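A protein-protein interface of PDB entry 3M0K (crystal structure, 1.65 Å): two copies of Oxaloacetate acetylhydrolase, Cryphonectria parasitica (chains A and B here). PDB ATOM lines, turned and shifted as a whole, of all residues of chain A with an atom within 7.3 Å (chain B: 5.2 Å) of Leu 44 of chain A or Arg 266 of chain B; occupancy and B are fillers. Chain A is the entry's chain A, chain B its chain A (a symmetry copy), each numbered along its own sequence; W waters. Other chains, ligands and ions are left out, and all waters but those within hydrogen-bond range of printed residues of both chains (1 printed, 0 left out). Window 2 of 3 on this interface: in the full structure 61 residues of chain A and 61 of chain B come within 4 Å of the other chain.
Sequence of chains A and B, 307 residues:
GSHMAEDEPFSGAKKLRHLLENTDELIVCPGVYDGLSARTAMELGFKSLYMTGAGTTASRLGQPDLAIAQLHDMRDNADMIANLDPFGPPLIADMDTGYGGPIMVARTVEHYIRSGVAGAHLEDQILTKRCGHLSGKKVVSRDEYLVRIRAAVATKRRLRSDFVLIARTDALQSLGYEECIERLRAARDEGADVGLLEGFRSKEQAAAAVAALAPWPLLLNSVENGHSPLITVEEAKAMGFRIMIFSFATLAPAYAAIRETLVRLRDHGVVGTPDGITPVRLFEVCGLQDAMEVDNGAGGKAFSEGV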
ATOM      1  N   VAL A  28     -23.789 -17.812  36.466  1.00  0.00           N
ATOM      2  CA  VAL A  28     -24.676 -18.565  35.586  1.00  0.00           C
ATOM      3  C   VAL A  28     -24.099 -19.931  35.266  1.00  0.00           C
ATOM      4  O   VAL A  28     -23.011 -20.031  34.696  1.00  0.00           O
ATOM      5  CB  VAL A  28     -24.919 -17.784  34.281  1.00  0.00           C
ATOM      6  CG1 VAL A  28     -25.656 -18.642  33.235  1.00  0.00           C
ATOM      7  CG2 VAL A  28     -25.668 -16.501  34.592  1.00  0.00           C
ATOM      8  N   ALA A  38     -20.866 -31.085  28.982  1.00  0.00           N
ATOM      9  CA  ALA A  38     -19.907 -30.307  29.755  1.00  0.00           C
ATOM     10  C   ALA A  38     -18.853 -29.659  28.850  1.00  0.00           C
ATOM     11  O   ALA A  38     -18.506 -28.495  29.031  1.00  0.00           O
ATOM     12  CB  ALA A  38     -19.245 -31.177  30.839  1.00  0.00           C
ATOM     13  N   ARG A  39     -18.350 -30.418  27.882  1.00  0.00           N
ATOM     14  CA  ARG A  39     -17.312 -29.894  26.996  1.00  0.00           C
ATOM     15  C   ARG A  39     -17.839 -28.711  26.192  1.00  0.00           C
ATOM     16  O   ARG A  39     -17.100 -27.768  25.925  1.00  0.00           O
ATOM     17  CB  ARG A  39     -16.774 -30.983  26.058  1.00  0.00           C
ATOM     18  CG  ARG A  39     -15.799 -31.967  26.711  1.00  0.00           C
ATOM     19  CD  ARG A  39     -14.434 -31.337  27.009  1.00  0.00           C
ATOM     20  NE  ARG A  39     -13.426 -32.379  27.245  1.00  0.00           N
ATOM     21  CZ  ARG A  39     -12.141 -32.155  27.491  1.00  0.00           C
ATOM     22  NH1 ARG A  39     -11.672 -30.914  27.554  1.00  0.00           N
ATOM     23  NH2 ARG A  39     -11.321 -33.187  27.689  1.00  0.00           N
ATOM     24  N   THR A  40     -19.113 -28.770  25.815  1.00  0.00           N
ATOM     25  CA  THR A  40     -19.742 -27.680  25.067  1.00  0.00           C
ATOM     26  C   THR A  40     -19.884 -26.413  25.911  1.00  0.00           C
ATOM     27  O   THR A  40     -19.593 -25.320  25.440  1.00  0.00           O
ATOM     28  CB  THR A  40     -21.091 -28.113  24.473  1.00  0.00           C
ATOM     29  OG1 THR A  40     -20.902 -29.314  23.721  1.00  0.00           O
ATOM     30  CG2 THR A  40     -21.656 -27.037  23.541  1.00  0.00           C
ATOM     31  N   ALA A  41     -20.303 -26.561  27.162  1.00  0.00           N
ATOM     32  CA  ALA A  41     -20.381 -25.424  28.065  1.00  0.00           C
ATOM     33  C   ALA A  41     -19.009 -24.791  28.240  1.00  0.00           C
ATOM     34  O   ALA A  41     -18.893 -23.572  28.299  1.00  0.00           O
ATOM     35  CB  ALA A  41     -20.945 -25.855  29.422  1.00  0.00           C
ATOM     36  N   MET A  42     -17.975 -25.629  28.326  1.00  0.00           N
ATOM     37  CA  MET A  42     -16.609 -25.138  28.497  1.00  0.00           C
ATOM     38  C   MET A  42     -16.115 -24.422  27.244  1.00  0.00           C
ATOM     39  O   MET A  42     -15.440 -23.395  27.335  1.00  0.00           O
ATOM     40  CB  MET A  42     -15.662 -26.283  28.864  1.00  0.00           C
ATOM     41  CG  MET A  42     -15.994 -26.975  30.181  1.00  0.00           C
ATOM     42  SD  MET A  42     -15.248 -28.630  30.280  1.00  0.00           S
ATOM     43  CE  MET A  42     -13.524 -28.206  30.476  1.00  0.00           C
ATOM     44  N   GLU A  43     -16.452 -24.979  26.085  1.00  0.00           N
ATOM     45  CA  GLU A  43     -16.101 -24.404  24.793  1.00  0.00           C
ATOM     46  C   GLU A  43     -16.610 -22.977  24.717  1.00  0.00           C
ATOM     47  O   GLU A  43     -15.954 -22.100  24.151  1.00  0.00           O
ATOM     48  CB  GLU A  43     -16.736 -25.236  23.666  1.00  0.00           C
ATOM     49  CG  GLU A  43     -16.420 -24.787  22.241  1.00  0.00           C
ATOM     50  CD  GLU A  43     -17.393 -25.347  21.208  1.00  0.00           C
ATOM     51  OE1 GLU A  43     -18.149 -26.282  21.528  1.00  0.00           O
ATOM     52  OE2 GLU A  43     -17.415 -24.841  20.064  1.00  0.00           O
ATOM     53  N   LEU A  44     -17.785 -22.749  25.294  1.00  0.00           N
ATOM     54  CA  LEU A  44     -18.456 -21.460  25.170  1.00  0.00           C
ATOM     55  C   LEU A  44     -18.086 -20.460  26.264  1.00  0.00           C
ATOM     56  O   LEU A  44     -18.552 -19.325  26.244  1.00  0.00           O
ATOM     57  CB  LEU A  44     -19.970 -21.658  25.127  1.00  0.00           C
ATOM     58  CG  LEU A  44     -20.448 -22.469  23.919  1.00  0.00           C
ATOM     59  CD1 LEU A  44     -21.925 -22.770  24.065  1.00  0.00           C
ATOM     60  CD2 LEU A  44     -20.167 -21.722  22.606  1.00  0.00           C
ATOM     61  N   GLY A  45     -17.275 -20.886  27.224  1.00  0.00           N
ATOM     62  CA  GLY A  45     -16.721 -19.974  28.205  1.00  0.00           C
ATOM     63  C   GLY A  45     -17.551 -19.719  29.448  1.00  0.00           C
ATOM     64  O   GLY A  45     -17.325 -18.725  30.145  1.00  0.00           O
ATOM     65  N   PHE A  46     -18.513 -20.590  29.744  1.00  0.00           N
ATOM     66  CA  PHE A  46     -19.249 -20.434  30.997  1.00  0.00           C
ATOM     67  C   PHE A  46     -18.279 -20.496  32.169  1.00  0.00           C
ATOM     68  O   PHE A  46     -17.312 -21.260  32.148  1.00  0.00           O
ATOM     69  CB  PHE A  46     -20.379 -21.456  31.136  1.00  0.00           C
ATOM     70  CG  PHE A  46     -21.551 -21.165  30.251  1.00  0.00           C
ATOM     71  CD1 PHE A  46     -22.605 -20.401  30.706  1.00  0.00           C
ATOM     72  CD2 PHE A  46     -21.574 -21.618  28.947  1.00  0.00           C
ATOM     73  CE1 PHE A  46     -23.680 -20.117  29.884  1.00  0.00           C
ATOM     74  CE2 PHE A  46     -22.647 -21.339  28.117  1.00  0.00           C
ATOM     75  CZ  PHE A  46     -23.692 -20.578  28.578  1.00  0.00           C
ATOM     76  N   LYS A  47     -18.543 -19.678  33.184  1.00  0.00           N
ATOM     77  CA  LYS A  47     -17.622 -19.502  34.298  1.00  0.00           C
ATOM     78  C   LYS A  47     -17.840 -20.545  35.385  1.00  0.00           C
ATOM     79  O   LYS A  47     -17.025 -20.695  36.288  1.00  0.00           O
ATOM     80  CB  LYS A  47     -17.771 -18.098  34.884  1.00  0.00           C
ATOM     81  CG  LYS A  47     -17.323 -16.999  33.936  1.00  0.00           C
ATOM     82  CD  LYS A  47     -17.342 -15.647  34.620  1.00  0.00           C
ATOM     83  CE  LYS A  47     -16.274 -15.558  35.705  1.00  0.00           C
ATOM     84  NZ  LYS A  47     -16.157 -14.173  36.244  1.00  0.00           N
ATOM     85  N   VAL A 233     -31.920 -14.312  32.982  1.00  0.00           N
ATOM     86  CA  VAL A 233     -30.693 -14.061  33.724  1.00  0.00           C
ATOM     87  C   VAL A 233     -30.706 -12.656  34.312  1.00  0.00           C
ATOM     88  O   VAL A 233     -30.353 -12.453  35.478  1.00  0.00           O
ATOM     89  CB  VAL A 233     -29.445 -14.266  32.842  1.00  0.00           C
ATOM     90  CG1 VAL A 233     -28.221 -13.627  33.476  1.00  0.00           C
ATOM     91  CG2 VAL A 233     -29.218 -15.758  32.591  1.00  0.00           C
ATOM     92  N   ARG B 259     -25.071 -26.902  21.766  1.00  0.00           N
ATOM     93  CA  ARG B 259     -24.272 -25.711  21.517  1.00  0.00           C
ATOM     94  C   ARG B 259     -25.149 -24.497  21.189  1.00  0.00           C
ATOM     95  O   ARG B 259     -24.975 -23.407  21.761  1.00  0.00           O
ATOM     96  CB  ARG B 259     -23.282 -25.965  20.387  1.00  0.00           C
ATOM     97  CG  ARG B 259     -22.243 -24.876  20.242  1.00  0.00           C
ATOM     98  CD  ARG B 259     -21.427 -25.039  18.978  1.00  0.00           C
ATOM     99  NE  ARG B 259     -20.163 -24.317  19.104  1.00  0.00           N
ATOM    100  CZ  ARG B 259     -20.049 -22.995  19.009  1.00  0.00           C
ATOM    101  NH1 ARG B 259     -21.122 -22.251  18.779  1.00  0.00           N
ATOM    102  NH2 ARG B 259     -18.860 -22.418  19.143  1.00  0.00           N
ATOM    103  N   THR B 261     -28.236 -23.997  21.954  1.00  0.00           N
ATOM    104  CA  THR B 261     -28.935 -23.619  23.173  1.00  0.00           C
ATOM    105  C   THR B 261     -28.054 -22.835  24.147  1.00  0.00           C
ATOM    106  O   THR B 261     -28.472 -21.808  24.677  1.00  0.00           O
ATOM    107  CB  THR B 261     -29.501 -24.856  23.858  1.00  0.00           C
ATOM    108  OG1 THR B 261     -30.452 -25.471  22.980  1.00  0.00           O
ATOM    109  CG2 THR B 261     -30.187 -24.476  25.168  1.00  0.00           C
ATOM    110  N   LEU B 262     -26.834 -23.309  24.379  1.00  0.00           N
ATOM    111  CA  LEU B 262     -25.952 -22.642  25.337  1.00  0.00           C
ATOM    112  C   LEU B 262     -25.509 -21.272  24.831  1.00  0.00           C
ATOM    113  O   LEU B 262     -25.320 -20.347  25.613  1.00  0.00           O
ATOM    114  CB  LEU B 262     -24.748 -23.527  25.667  1.00  0.00           C
ATOM    115  CG  LEU B 262     -25.102 -24.750  26.519  1.00  0.00           C
ATOM    116  CD1 LEU B 262     -23.830 -25.481  26.946  1.00  0.00           C
ATOM    117  CD2 LEU B 262     -25.902 -24.336  27.728  1.00  0.00           C
ATOM    118  N   VAL B 263     -25.364 -21.150  23.518  1.00  0.00           N
ATOM    119  CA  VAL B 263     -25.061 -19.866  22.918  1.00  0.00           C
ATOM    120  C   VAL B 263     -26.207 -18.890  23.173  1.00  0.00           C
ATOM    121  O   VAL B 263     -25.974 -17.761  23.569  1.00  0.00           O
ATOM    122  CB  VAL B 263     -24.772 -19.975  21.407  1.00  0.00           C
ATOM    123  CG1 VAL B 263     -24.806 -18.581  20.771  1.00  0.00           C
ATOM    124  CG2 VAL B 263     -23.420 -20.632  21.176  1.00  0.00           C
ATOM    125  N   ARG B 264     -27.440 -19.345  22.976  1.00  0.00           N
ATOM    126  CA  ARG B 264     -28.620 -18.537  23.306  1.00  0.00           C
ATOM    127  C   ARG B 264     -28.656 -18.160  24.789  1.00  0.00           C
ATOM    128  O   ARG B 264     -28.947 -17.018  25.154  1.00  0.00           O
ATOM    129  CB  ARG B 264     -29.900 -19.293  22.933  1.00  0.00           C
ATOM    130  CG  ARG B 264     -31.193 -18.575  23.284  1.00  0.00           C
ATOM    131  CD  ARG B 264     -32.410 -19.395  22.872  1.00  0.00           C
ATOM    132  NE  ARG B 264     -32.274 -19.903  21.507  1.00  0.00           N
ATOM    133  CZ  ARG B 264     -32.317 -21.189  21.168  1.00  0.00           C
ATOM    134  NH1 ARG B 264     -32.515 -22.128  22.088  1.00  0.00           N
ATOM    135  NH2 ARG B 264     -32.170 -21.536  19.898  1.00  0.00           N
ATOM    136  N   LEU B 265     -28.364 -19.125  25.651  1.00  0.00           N
ATOM    137  CA  LEU B 265     -28.344 -18.845  27.081  1.00  0.00           C
ATOM    138  C   LEU B 265     -27.293 -17.775  27.363  1.00  0.00           C
ATOM    139  O   LEU B 265     -27.544 -16.806  28.074  1.00  0.00           O
ATOM    140  CB  LEU B 265     -28.041 -20.121  27.862  1.00  0.00           C
ATOM    141  CG  LEU B 265     -27.838 -19.929  29.362  1.00  0.00           C
ATOM    142  CD1 LEU B 265     -28.982 -19.101  29.935  1.00  0.00           C
ATOM    143  CD2 LEU B 265     -27.735 -21.283  30.063  1.00  0.00           C
ATOM    144  N   ARG B 266     -26.114 -17.951  26.790  1.00  0.00           N
ATOM    145  CA  ARG B 266     -25.021 -17.025  27.025  1.00  0.00           C
ATOM    146  C   ARG B 266     -25.357 -15.610  26.570  1.00  0.00           C
ATOM    147  O   ARG B 266     -25.094 -14.643  27.284  1.00  0.00           O
ATOM    148  CB  ARG B 266     -23.755 -17.499  26.319  1.00  0.00           C
ATOM    149  CG  ARG B 266     -22.530 -16.692  26.713  1.00  0.00           C
ATOM    150  CD  ARG B 266     -21.345 -17.064  25.856  1.00  0.00           C
ATOM    151  NE  ARG B 266     -21.626 -16.797  24.451  1.00  0.00           N
ATOM    152  CZ  ARG B 266     -20.906 -17.275  23.443  1.00  0.00           C
ATOM    153  NH1 ARG B 266     -19.861 -18.059  23.684  1.00  0.00           N
ATOM    154  NH2 ARG B 266     -21.234 -16.971  22.196  1.00  0.00           N
ATOM    155  N   ASP B 267     -25.950 -15.491  25.388  1.00  0.00           N
ATOM    156  CA  ASP B 267     -26.160 -14.182  24.774  1.00  0.00           C
ATOM    157  C   ASP B 267     -27.480 -13.502  25.135  1.00  0.00           C
ATOM    158  O   ASP B 267     -27.576 -12.265  25.094  1.00  0.00           O
ATOM    159  CB  ASP B 267     -26.044 -14.298  23.258  1.00  0.00           C
ATOM    160  CG  ASP B 267     -24.654 -14.671  22.810  1.00  0.00           C
ATOM    161  OD1 ASP B 267     -23.716 -14.577  23.628  1.00  0.00           O
ATOM    162  OD2 ASP B 267     -24.511 -15.059  21.635  1.00  0.00           O
ATOM    163  N   HIS B 268     -28.485 -14.298  25.490  1.00  0.00           N
ATOM    164  CA  HIS B 268     -29.844 -13.792  25.682  1.00  0.00           C
ATOM    165  C   HIS B 268     -30.468 -14.165  27.023  1.00  0.00           C
ATOM    166  O   HIS B 268     -31.610 -13.808  27.302  1.00  0.00           O
ATOM    167  CB  HIS B 268     -30.748 -14.291  24.560  1.00  0.00           C
ATOM    168  CG  HIS B 268     -30.319 -13.838  23.203  1.00  0.00           C
ATOM    169  ND1 HIS B 268     -30.382 -12.519  22.813  1.00  0.00           N
ATOM    170  CD2 HIS B 268     -29.817 -14.524  22.149  1.00  0.00           C
ATOM    171  CE1 HIS B 268     -29.939 -12.410  21.571  1.00  0.00           C
ATOM    172  NE2 HIS B 268     -29.589 -13.610  21.149  1.00  0.00           N
ATOM    173  N   GLY B 269     -29.735 -14.905  27.845  1.00  0.00           N
ATOM    174  CA  GLY B 269     -30.204 -15.217  29.182  1.00  0.00           C
ATOM    175  C   GLY B 269     -31.411 -16.128  29.284  1.00  0.00           C
ATOM    176  O   GLY B 269     -32.032 -16.215  30.341  1.00  0.00           O
HETATM  177  O   HOH W   1     -15.783 -23.179  19.144  1.00  0.00           O
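The backbone carbonyl oxygen of Leu 44 of chain A sits at hydrogen-bond distance from the guanidinium group of Arg 266 of chain B, at 3.1 Å.
O of Gly 269 of chain B is in hydrogen-bond range of N of Val 233 of chain A, 3.3 Å away.
The guanidinium group of Arg 259 of chain B lies within salt-bridge range of the side-chain carboxylate of Glu 43 of chain A (3.0 Å).
Among the printed residues, merely in contact across the chains: Leu 44 of chain A with Leu 262 of chain B, Phe 46 of chain A with Leu 262 of chain B, Thr 40 of chain A with Arg 259 of chain B, Ala 41 of chain A with Leu 262 of chain B, Leu 44 of chain A with Val 263 of chain B, Leu 44 of chain A with Arg 259 of chain B and Phe 46 of chain A with Arg 266 of chain B.
Leu 44 of chain A touches just these residues of chain B: Arg 259 (3.8 Å), Leu 262 (3.3 Å), Val 263 (3.7 Å) and Arg 266 (3.1 Å).
Of the printed residues of chain A, Arg 266 of chain B touches Leu 44 (3.1 Å) and Phe 46 (3.8 Å).
Of the printed residues of chain B, Val 233 of chain A touches Gly 269.
Of the printed residues of chain A, Val 263 of chain B touches Leu 44.
Of the printed residues of chain A, Leu 262 of chain B touches Ala 41, Leu 44 and Phe 46.
Of the printed residues of chain B, Thr 40 of chain A touches Arg 259.
The nearest residue of chain A that does not touch Arg 266 of chain B is Gly 45 of chain A (5.2 Å).
Water W1 bridges OE2 of Glu 43 of chain A (2.5 Å) and NH2 of Arg 259 of chain B (3.2 Å).
No position is printed for both chains.
Of the 10 pairs that touch across the chains among the printed residues, none has its exchanged pair printed and touching as well.
Printed residues of chain A that touch a printed residue of chain B: Thr 40, Ala 41, Glu 43, Leu 44, Phe 46 and Val 233.
Among the printed residues, 10 pairs touch across the chains.
Among the printed residues, Asp or Glu carboxylates within 4 Å of a Lys or Arg side-chain nitrogen of the other chain: Glu 43 of chain A with Arg 259 of chain B.
NE of Arg 266 of chain B lies within salt-bridge range of OD1 of Asp 267 of chain B (3.2 Å).
The backbone carbonyl oxygen of Ala 41 of chain A is in hydrogen-bond range of the backbone NH of Phe 46 of chain A (3.3 Å).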
